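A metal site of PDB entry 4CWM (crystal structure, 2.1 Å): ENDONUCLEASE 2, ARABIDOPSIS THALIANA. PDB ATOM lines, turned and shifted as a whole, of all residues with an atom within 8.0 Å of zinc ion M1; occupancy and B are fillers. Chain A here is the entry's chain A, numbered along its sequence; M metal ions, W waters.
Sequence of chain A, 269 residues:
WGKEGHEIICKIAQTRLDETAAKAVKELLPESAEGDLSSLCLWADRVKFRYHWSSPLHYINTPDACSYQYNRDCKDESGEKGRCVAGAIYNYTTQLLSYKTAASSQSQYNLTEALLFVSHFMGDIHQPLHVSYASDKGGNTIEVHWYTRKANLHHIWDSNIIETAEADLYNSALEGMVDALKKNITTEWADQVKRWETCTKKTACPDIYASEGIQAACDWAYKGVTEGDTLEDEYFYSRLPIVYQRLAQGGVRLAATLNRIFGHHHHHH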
ATOM      1  N   TRP A   1     -26.054   2.555 -30.777  1.00  0.00           N
ATOM      2  CA  TRP A   1     -27.148   3.121 -31.611  1.00  0.00           C
ATOM      3  C   TRP A   1     -28.510   2.909 -30.999  1.00  0.00           C
ATOM      4  O   TRP A   1     -28.708   2.049 -30.141  1.00  0.00           O
ATOM      5  CB  TRP A   1     -27.210   2.462 -32.992  1.00  0.00           C
ATOM      6  CG  TRP A   1     -25.910   2.350 -33.697  1.00  0.00           C
ATOM      7  CD1 TRP A   1     -25.038   1.308 -33.631  1.00  0.00           C
ATOM      8  CD2 TRP A   1     -25.353   3.296 -34.605  1.00  0.00           C
ATOM      9  NE1 TRP A   1     -23.966   1.546 -34.447  1.00  0.00           N
ATOM     10  CE2 TRP A   1     -24.141   2.773 -35.059  1.00  0.00           C
ATOM     11  CE3 TRP A   1     -25.760   4.537 -35.086  1.00  0.00           C
ATOM     12  CZ2 TRP A   1     -23.320   3.436 -35.963  1.00  0.00           C
ATOM     13  CZ3 TRP A   1     -24.956   5.216 -35.997  1.00  0.00           C
ATOM     14  CH2 TRP A   1     -23.750   4.661 -36.413  1.00  0.00           C
ATOM     15  N   GLY A   2     -29.465   3.670 -31.476  1.00  0.00           N
ATOM     16  CA  GLY A   2     -30.830   3.448 -31.109  1.00  0.00           C
ATOM     17  C   GLY A   2     -31.319   2.301 -31.962  1.00  0.00           C
ATOM     18  O   GLY A   2     -30.536   1.606 -32.620  1.00  0.00           O
ATOM     19  N   HIS A   6     -29.380  -0.406 -34.962  1.00  0.00           N
ATOM     20  CA  HIS A   6     -29.181  -1.833 -34.671  1.00  0.00           C
ATOM     21  C   HIS A   6     -29.959  -2.756 -35.619  1.00  0.00           C
ATOM     22  O   HIS A   6     -29.489  -3.849 -35.975  1.00  0.00           O
ATOM     23  CB  HIS A   6     -29.553  -2.132 -33.204  1.00  0.00           C
ATOM     24  CG  HIS A   6     -28.519  -1.661 -32.220  1.00  0.00           C
ATOM     25  ND1 HIS A   6     -27.269  -2.222 -32.136  1.00  0.00           N
ATOM     26  CD2 HIS A   6     -28.552  -0.672 -31.300  1.00  0.00           C
ATOM     27  CE1 HIS A   6     -26.574  -1.612 -31.187  1.00  0.00           C
ATOM     28  NE2 HIS A   6     -27.333  -0.674 -30.672  1.00  0.00           N
ATOM     29  N   ASP A  45     -29.973  -3.404 -24.688  1.00  0.00           N
ATOM     30  CA  ASP A  45     -30.230  -2.071 -24.107  1.00  0.00           C
ATOM     31  C   ASP A  45     -31.298  -2.151 -22.997  1.00  0.00           C
ATOM     32  O   ASP A  45     -31.441  -1.226 -22.201  1.00  0.00           O
ATOM     33  CB  ASP A  45     -30.637  -1.047 -25.168  1.00  0.00           C
ATOM     34  CG  ASP A  45     -29.434  -0.371 -25.866  1.00  0.00           C
ATOM     35  OD1 ASP A  45     -28.312  -0.293 -25.305  1.00  0.00           O
ATOM     36  OD2 ASP A  45     -29.647   0.108 -26.998  1.00  0.00           O
ATOM     37  N   LYS A  48     -29.618  -3.315 -18.986  1.00  0.00           N
ATOM     38  CA  LYS A  48     -28.550  -2.578 -18.292  1.00  0.00           C
ATOM     39  C   LYS A  48     -28.672  -2.539 -16.752  1.00  0.00           C
ATOM     40  O   LYS A  48     -27.685  -2.390 -16.071  1.00  0.00           O
ATOM     41  CB  LYS A  48     -28.436  -1.135 -18.802  1.00  0.00           C
ATOM     42  CG  LYS A  48     -28.110  -1.024 -20.286  1.00  0.00           C
ATOM     43  CD  LYS A  48     -27.818   0.409 -20.670  1.00  0.00           C
ATOM     44  CE  LYS A  48     -27.458   0.539 -22.115  1.00  0.00           C
ATOM     45  NZ  LYS A  48     -27.470   1.987 -22.480  1.00  0.00           N
ATOM     46  N   HIS A  58     -21.350  -1.401 -23.208  1.00  0.00           N
ATOM     47  CA  HIS A  58     -21.915  -0.795 -24.401  1.00  0.00           C
ATOM     48  C   HIS A  58     -20.985   0.236 -25.063  1.00  0.00           C
ATOM     49  O   HIS A  58     -21.264   0.676 -26.155  1.00  0.00           O
ATOM     50  CB  HIS A  58     -23.231  -0.147 -24.070  1.00  0.00           C
ATOM     51  CG  HIS A  58     -24.317  -1.125 -23.751  1.00  0.00           C
ATOM     52  ND1 HIS A  58     -25.362  -1.372 -24.593  1.00  0.00           N
ATOM     53  CD2 HIS A  58     -24.508  -1.928 -22.677  1.00  0.00           C
ATOM     54  CE1 HIS A  58     -26.162  -2.294 -24.068  1.00  0.00           C
ATOM     55  NE2 HIS A  58     -25.657  -2.645 -22.901  1.00  0.00           N
ATOM     56  N   TYR A  59     -19.891   0.623 -24.406  1.00  0.00           N
ATOM     57  CA  TYR A  59     -19.076   1.767 -24.885  1.00  0.00           C
ATOM     58  C   TYR A  59     -17.628   1.683 -24.433  1.00  0.00           C
ATOM     59  O   TYR A  59     -17.264   0.773 -23.722  1.00  0.00           O
ATOM     60  CB  TYR A  59     -19.680   3.103 -24.396  1.00  0.00           C
ATOM     61  CG  TYR A  59     -19.800   3.143 -22.890  1.00  0.00           C
ATOM     62  CD1 TYR A  59     -18.718   3.545 -22.079  1.00  0.00           C
ATOM     63  CD2 TYR A  59     -20.970   2.704 -22.262  1.00  0.00           C
ATOM     64  CE1 TYR A  59     -18.836   3.574 -20.690  1.00  0.00           C
ATOM     65  CE2 TYR A  59     -21.095   2.724 -20.881  1.00  0.00           C
ATOM     66  CZ  TYR A  59     -20.025   3.145 -20.100  1.00  0.00           C
ATOM     67  OH  TYR A  59     -20.195   3.112 -18.738  1.00  0.00           O
ATOM     68  N   HIS A 120     -25.469  -6.961 -30.558  1.00  0.00           N
ATOM     69  CA  HIS A 120     -25.651  -5.585 -30.107  1.00  0.00           C
ATOM     70  C   HIS A 120     -24.350  -4.821 -30.001  1.00  0.00           C
ATOM     71  O   HIS A 120     -24.243  -3.696 -30.453  1.00  0.00           O
ATOM     72  CB  HIS A 120     -26.324  -5.595 -28.769  1.00  0.00           C
ATOM     73  CG  HIS A 120     -26.671  -4.230 -28.297  1.00  0.00           C
ATOM     74  ND1 HIS A 120     -27.798  -3.567 -28.708  1.00  0.00           N
ATOM     75  CD2 HIS A 120     -26.027  -3.403 -27.459  1.00  0.00           C
ATOM     76  CE1 HIS A 120     -27.840  -2.385 -28.129  1.00  0.00           C
ATOM     77  NE2 HIS A 120     -26.758  -2.250 -27.386  1.00  0.00           N
ATOM     78  N   ASP A 124     -22.749  -1.386 -31.501  1.00  0.00           N
ATOM     79  CA  ASP A 124     -22.339  -0.266 -30.627  1.00  0.00           C
ATOM     80  C   ASP A 124     -20.911   0.123 -30.820  1.00  0.00           C
ATOM     81  O   ASP A 124     -20.662   1.299 -30.815  1.00  0.00           O
ATOM     82  CB  ASP A 124     -22.561  -0.537 -29.144  1.00  0.00           C
ATOM     83  CG  ASP A 124     -23.929  -0.120 -28.672  1.00  0.00           C
ATOM     84  OD1 ASP A 124     -24.729   0.314 -29.476  1.00  0.00           O
ATOM     85  OD2 ASP A 124     -24.209  -0.268 -27.493  1.00  0.00           O
ATOM     86  N   GLN A 127     -20.636   2.758 -33.447  1.00  0.00           N
ATOM     87  CA  GLN A 127     -21.100   4.117 -33.144  1.00  0.00           C
ATOM     88  C   GLN A 127     -19.893   4.960 -32.698  1.00  0.00           C
ATOM     89  O   GLN A 127     -19.263   4.649 -31.679  1.00  0.00           O
ATOM     90  CB  GLN A 127     -22.195   4.111 -32.054  1.00  0.00           C
ATOM     91  CG  GLN A 127     -23.344   5.128 -32.279  1.00  0.00           C
ATOM     92  CD  GLN A 127     -22.979   6.553 -31.926  1.00  0.00           C
ATOM     93  OE1 GLN A 127     -22.016   7.127 -32.434  1.00  0.00           O
ATOM     94  NE2 GLN A 127     -23.780   7.154 -31.067  1.00  0.00           N
ATOM     95  N   LEU A 129     -19.503   7.777 -31.220  1.00  0.00           N
ATOM     96  CA  LEU A 129     -19.627   8.283 -29.870  1.00  0.00           C
ATOM     97  C   LEU A 129     -19.813   7.221 -28.791  1.00  0.00           C
ATOM     98  O   LEU A 129     -19.905   7.563 -27.618  1.00  0.00           O
ATOM     99  CB  LEU A 129     -20.720   9.350 -29.788  1.00  0.00           C
ATOM    100  CG  LEU A 129     -20.355  10.602 -30.590  1.00  0.00           C
ATOM    101  CD1 LEU A 129     -21.471  11.639 -30.529  1.00  0.00           C
ATOM    102  CD2 LEU A 129     -19.041  11.203 -30.073  1.00  0.00           C
ATOM    103  N   HIS A 130     -19.811   5.937 -29.150  1.00  0.00           N
ATOM    104  CA  HIS A 130     -19.715   4.860 -28.125  1.00  0.00           C
ATOM    105  C   HIS A 130     -18.256   4.508 -27.852  1.00  0.00           C
ATOM    106  O   HIS A 130     -17.969   3.576 -27.056  1.00  0.00           O
ATOM    107  CB  HIS A 130     -20.454   3.601 -28.556  1.00  0.00           C
ATOM    108  CG  HIS A 130     -21.888   3.609 -28.198  1.00  0.00           C
ATOM    109  ND1 HIS A 130     -22.411   2.786 -27.241  1.00  0.00           N
ATOM    110  CD2 HIS A 130     -22.906   4.408 -28.602  1.00  0.00           C
ATOM    111  CE1 HIS A 130     -23.698   3.073 -27.066  1.00  0.00           C
ATOM    112  NE2 HIS A 130     -24.029   4.035 -27.903  1.00  0.00           N
ATOM    113  N   LYS A 137     -18.856  12.345 -21.607  1.00  0.00           N
ATOM    114  CA  LYS A 137     -19.588  11.086 -21.621  1.00  0.00           C
ATOM    115  C   LYS A 137     -20.034  10.662 -23.009  1.00  0.00           C
ATOM    116  O   LYS A 137     -21.194  10.367 -23.230  1.00  0.00           O
ATOM    117  CB  LYS A 137     -20.796  11.164 -20.690  1.00  0.00           C
ATOM    118  CG  LYS A 137     -20.466  11.113 -19.207  1.00  0.00           C
ATOM    119  CD  LYS A 137     -21.706  10.749 -18.378  1.00  0.00           C
ATOM    120  CE  LYS A 137     -21.319  10.049 -17.074  1.00  0.00           C
ATOM    121  NZ  LYS A 137     -21.053  11.002 -15.975  1.00  0.00           N
ATOM    122  N   GLY A 138     -19.110  10.658 -23.957  1.00  0.00           N
ATOM    123  CA  GLY A 138     -19.426  10.210 -25.306  1.00  0.00           C
ATOM    124  C   GLY A 138     -20.379  11.143 -26.018  1.00  0.00           C
ATOM    125  O   GLY A 138     -21.116  10.734 -26.918  1.00  0.00           O
ATOM    126  N   ASN A 140     -22.952  12.836 -24.636  1.00  0.00           N
ATOM    127  CA  ASN A 140     -24.217  13.021 -23.942  1.00  0.00           C
ATOM    128  C   ASN A 140     -24.391  14.356 -23.220  1.00  0.00           C
ATOM    129  O   ASN A 140     -25.523  14.777 -22.968  1.00  0.00           O
ATOM    130  CB  ASN A 140     -24.433  11.941 -22.892  1.00  0.00           C
ATOM    131  CG  ASN A 140     -24.930  10.657 -23.479  1.00  0.00           C
ATOM    132  OD1 ASN A 140     -26.132  10.491 -23.709  1.00  0.00           O
ATOM    133  ND2 ASN A 140     -24.022   9.718 -23.718  1.00  0.00           N
ATOM    134  N   ASN A 152     -28.899  15.953 -27.350  1.00  0.00           N
ATOM    135  CA  ASN A 152     -27.457  15.903 -27.114  1.00  0.00           C
ATOM    136  C   ASN A 152     -26.736  15.282 -28.295  1.00  0.00           C
ATOM    137  O   ASN A 152     -27.345  14.563 -29.093  1.00  0.00           O
ATOM    138  CB  ASN A 152     -27.115  15.224 -25.805  1.00  0.00           C
ATOM    139  CG  ASN A 152     -27.407  13.771 -25.818  1.00  0.00           C
ATOM    140  OD1 ASN A 152     -26.674  12.983 -26.404  1.00  0.00           O
ATOM    141  ND2 ASN A 152     -28.494  13.390 -25.175  1.00  0.00           N
ATOM    142  N   HIS A 154     -24.695  12.906 -28.506  1.00  0.00           N
ATOM    143  CA  HIS A 154     -24.634  11.462 -28.537  1.00  0.00           C
ATOM    144  C   HIS A 154     -25.886  10.946 -29.216  1.00  0.00           C
ATOM    145  O   HIS A 154     -25.815  10.088 -30.089  1.00  0.00           O
ATOM    146  CB  HIS A 154     -24.556  10.885 -27.116  1.00  0.00           C
ATOM    147  CG  HIS A 154     -24.432   9.409 -27.082  1.00  0.00           C
ATOM    148  ND1 HIS A 154     -23.208   8.775 -27.141  1.00  0.00           N
ATOM    149  CD2 HIS A 154     -25.361   8.440 -27.051  1.00  0.00           C
ATOM    150  CE1 HIS A 154     -23.402   7.468 -27.164  1.00  0.00           C
ATOM    151  NE2 HIS A 154     -24.701   7.239 -27.124  1.00  0.00           N
ATOM    152  N   HIS A 155     -27.044  11.466 -28.771  1.00  0.00           N
ATOM    153  CA  HIS A 155     -28.332  11.037 -29.273  1.00  0.00           C
ATOM    154  C   HIS A 155     -28.468  11.298 -30.789  1.00  0.00           C
ATOM    155  O   HIS A 155     -29.044  10.492 -31.526  1.00  0.00           O
ATOM    156  CB  HIS A 155     -29.466  11.737 -28.545  1.00  0.00           C
ATOM    157  CG  HIS A 155     -30.806  11.112 -28.780  1.00  0.00           C
ATOM    158  ND1 HIS A 155     -31.751  11.655 -29.626  1.00  0.00           N
ATOM    159  CD2 HIS A 155     -31.360   9.983 -28.284  1.00  0.00           C
ATOM    160  CE1 HIS A 155     -32.829  10.898 -29.636  1.00  0.00           C
ATOM    161  NE2 HIS A 155     -32.627   9.877 -28.808  1.00  0.00           N
ATOM    162  N   TRP A 157     -26.162  11.074 -32.947  1.00  0.00           N
ATOM    163  CA  TRP A 157     -25.474   9.965 -33.621  1.00  0.00           C
ATOM    164  C   TRP A 157     -26.148   8.601 -33.432  1.00  0.00           C
ATOM    165  O   TRP A 157     -26.133   7.769 -34.339  1.00  0.00           O
ATOM    166  CB  TRP A 157     -23.999   9.907 -33.236  1.00  0.00           C
ATOM    167  CG  TRP A 157     -23.236  10.950 -33.997  1.00  0.00           C
ATOM    168  CD1 TRP A 157     -23.234  12.298 -33.765  1.00  0.00           C
ATOM    169  CD2 TRP A 157     -22.477  10.732 -35.171  1.00  0.00           C
ATOM    170  NE1 TRP A 157     -22.447  12.921 -34.705  1.00  0.00           N
ATOM    171  CE2 TRP A 157     -21.984  11.988 -35.592  1.00  0.00           C
ATOM    172  CE3 TRP A 157     -22.145   9.601 -35.922  1.00  0.00           C
ATOM    173  CZ2 TRP A 157     -21.192  12.130 -36.710  1.00  0.00           C
ATOM    174  CZ3 TRP A 157     -21.345   9.753 -37.033  1.00  0.00           C
ATOM    175  CH2 TRP A 157     -20.878  11.007 -37.422  1.00  0.00           C
ATOM    176  N   ASP A 158     -26.748   8.366 -32.260  1.00  0.00           N
ATOM    177  CA  ASP A 158     -27.530   7.128 -32.031  1.00  0.00           C
ATOM    178  C   ASP A 158     -28.725   7.004 -32.957  1.00  0.00           C
ATOM    179  O   ASP A 158     -28.958   5.937 -33.518  1.00  0.00           O
ATOM    180  CB  ASP A 158     -28.047   7.064 -30.597  1.00  0.00           C
ATOM    181  CG  ASP A 158     -27.053   6.476 -29.636  1.00  0.00           C
ATOM    182  OD1 ASP A 158     -26.052   5.918 -30.102  1.00  0.00           O
ATOM    183  OD2 ASP A 158     -27.286   6.536 -28.400  1.00  0.00           O
ATOM    184  N   SER A 159     -29.465   8.115 -33.092  1.00  0.00           N
ATOM    185  CA  SER A 159     -30.794   8.131 -33.680  1.00  0.00           C
ATOM    186  C   SER A 159     -31.107   9.224 -34.710  1.00  0.00           C
ATOM    187  O   SER A 159     -31.595   8.897 -35.811  1.00  0.00           O
ATOM    188  CB  SER A 159     -31.805   8.287 -32.563  1.00  0.00           C
ATOM    189  OG  SER A 159     -31.639   7.237 -31.654  1.00  0.00           O
HETATM  190 ZN    ZN M   1     -25.645   5.417 -27.556  1.00  0.00          ZN
HETATM  191 ZN    ZN M   2     -26.749   1.000 -29.557  1.00  0.00          ZN
HETATM  192 ZN    ZN M   3     -26.180  -0.194 -26.364  1.00  0.00          ZN
HETATM  193  O   HOH W   1     -26.927   3.725 -27.646  1.00  0.00           O
HETATM  194  O   HOH W   2     -26.013   4.966 -25.654  1.00  0.00           O
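Zinc ion M1 is bound by water W2, NE2 of His 154, water W1, NE2 of His 130 and OD2 of Asp 158. Slightly farther from zinc ion M1 lies the side-chain carboxylate (OD1) of Asp 158 (2.6 Å).
The backbone NH (N) of Gly 2 lies within hydrogen-bond range of the backbone carbonyl oxygen (O) of Asp 158, at 3.1 Å. The backbone NH (N) of Trp 1 sits close to the side-chain carboxylate (OD1) of Asp 158 (3.4 Å). The backbone carbonyl oxygen of Gly 138 sits at hydrogen-bond distance from a ring nitrogen (ND1) of His 154. The backbone NH (N) of His 154 lies within hydrogen-bond range of the side-chain amide oxygen (OD1) of Asn 152, at 2.9 Å. A ring nitrogen (ND1) of His 130 sits at hydrogen-bond distance from the backbone carbonyl oxygen (O) of His 58 (2.6 Å). OD1 of Asp 158 lies within hydrogen-bond range of NE2 of Gln 127, 2.8 Å away.
Three residues have an atom within 4 Å of zinc ion M1: His 130, His 154 and Asp 158.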
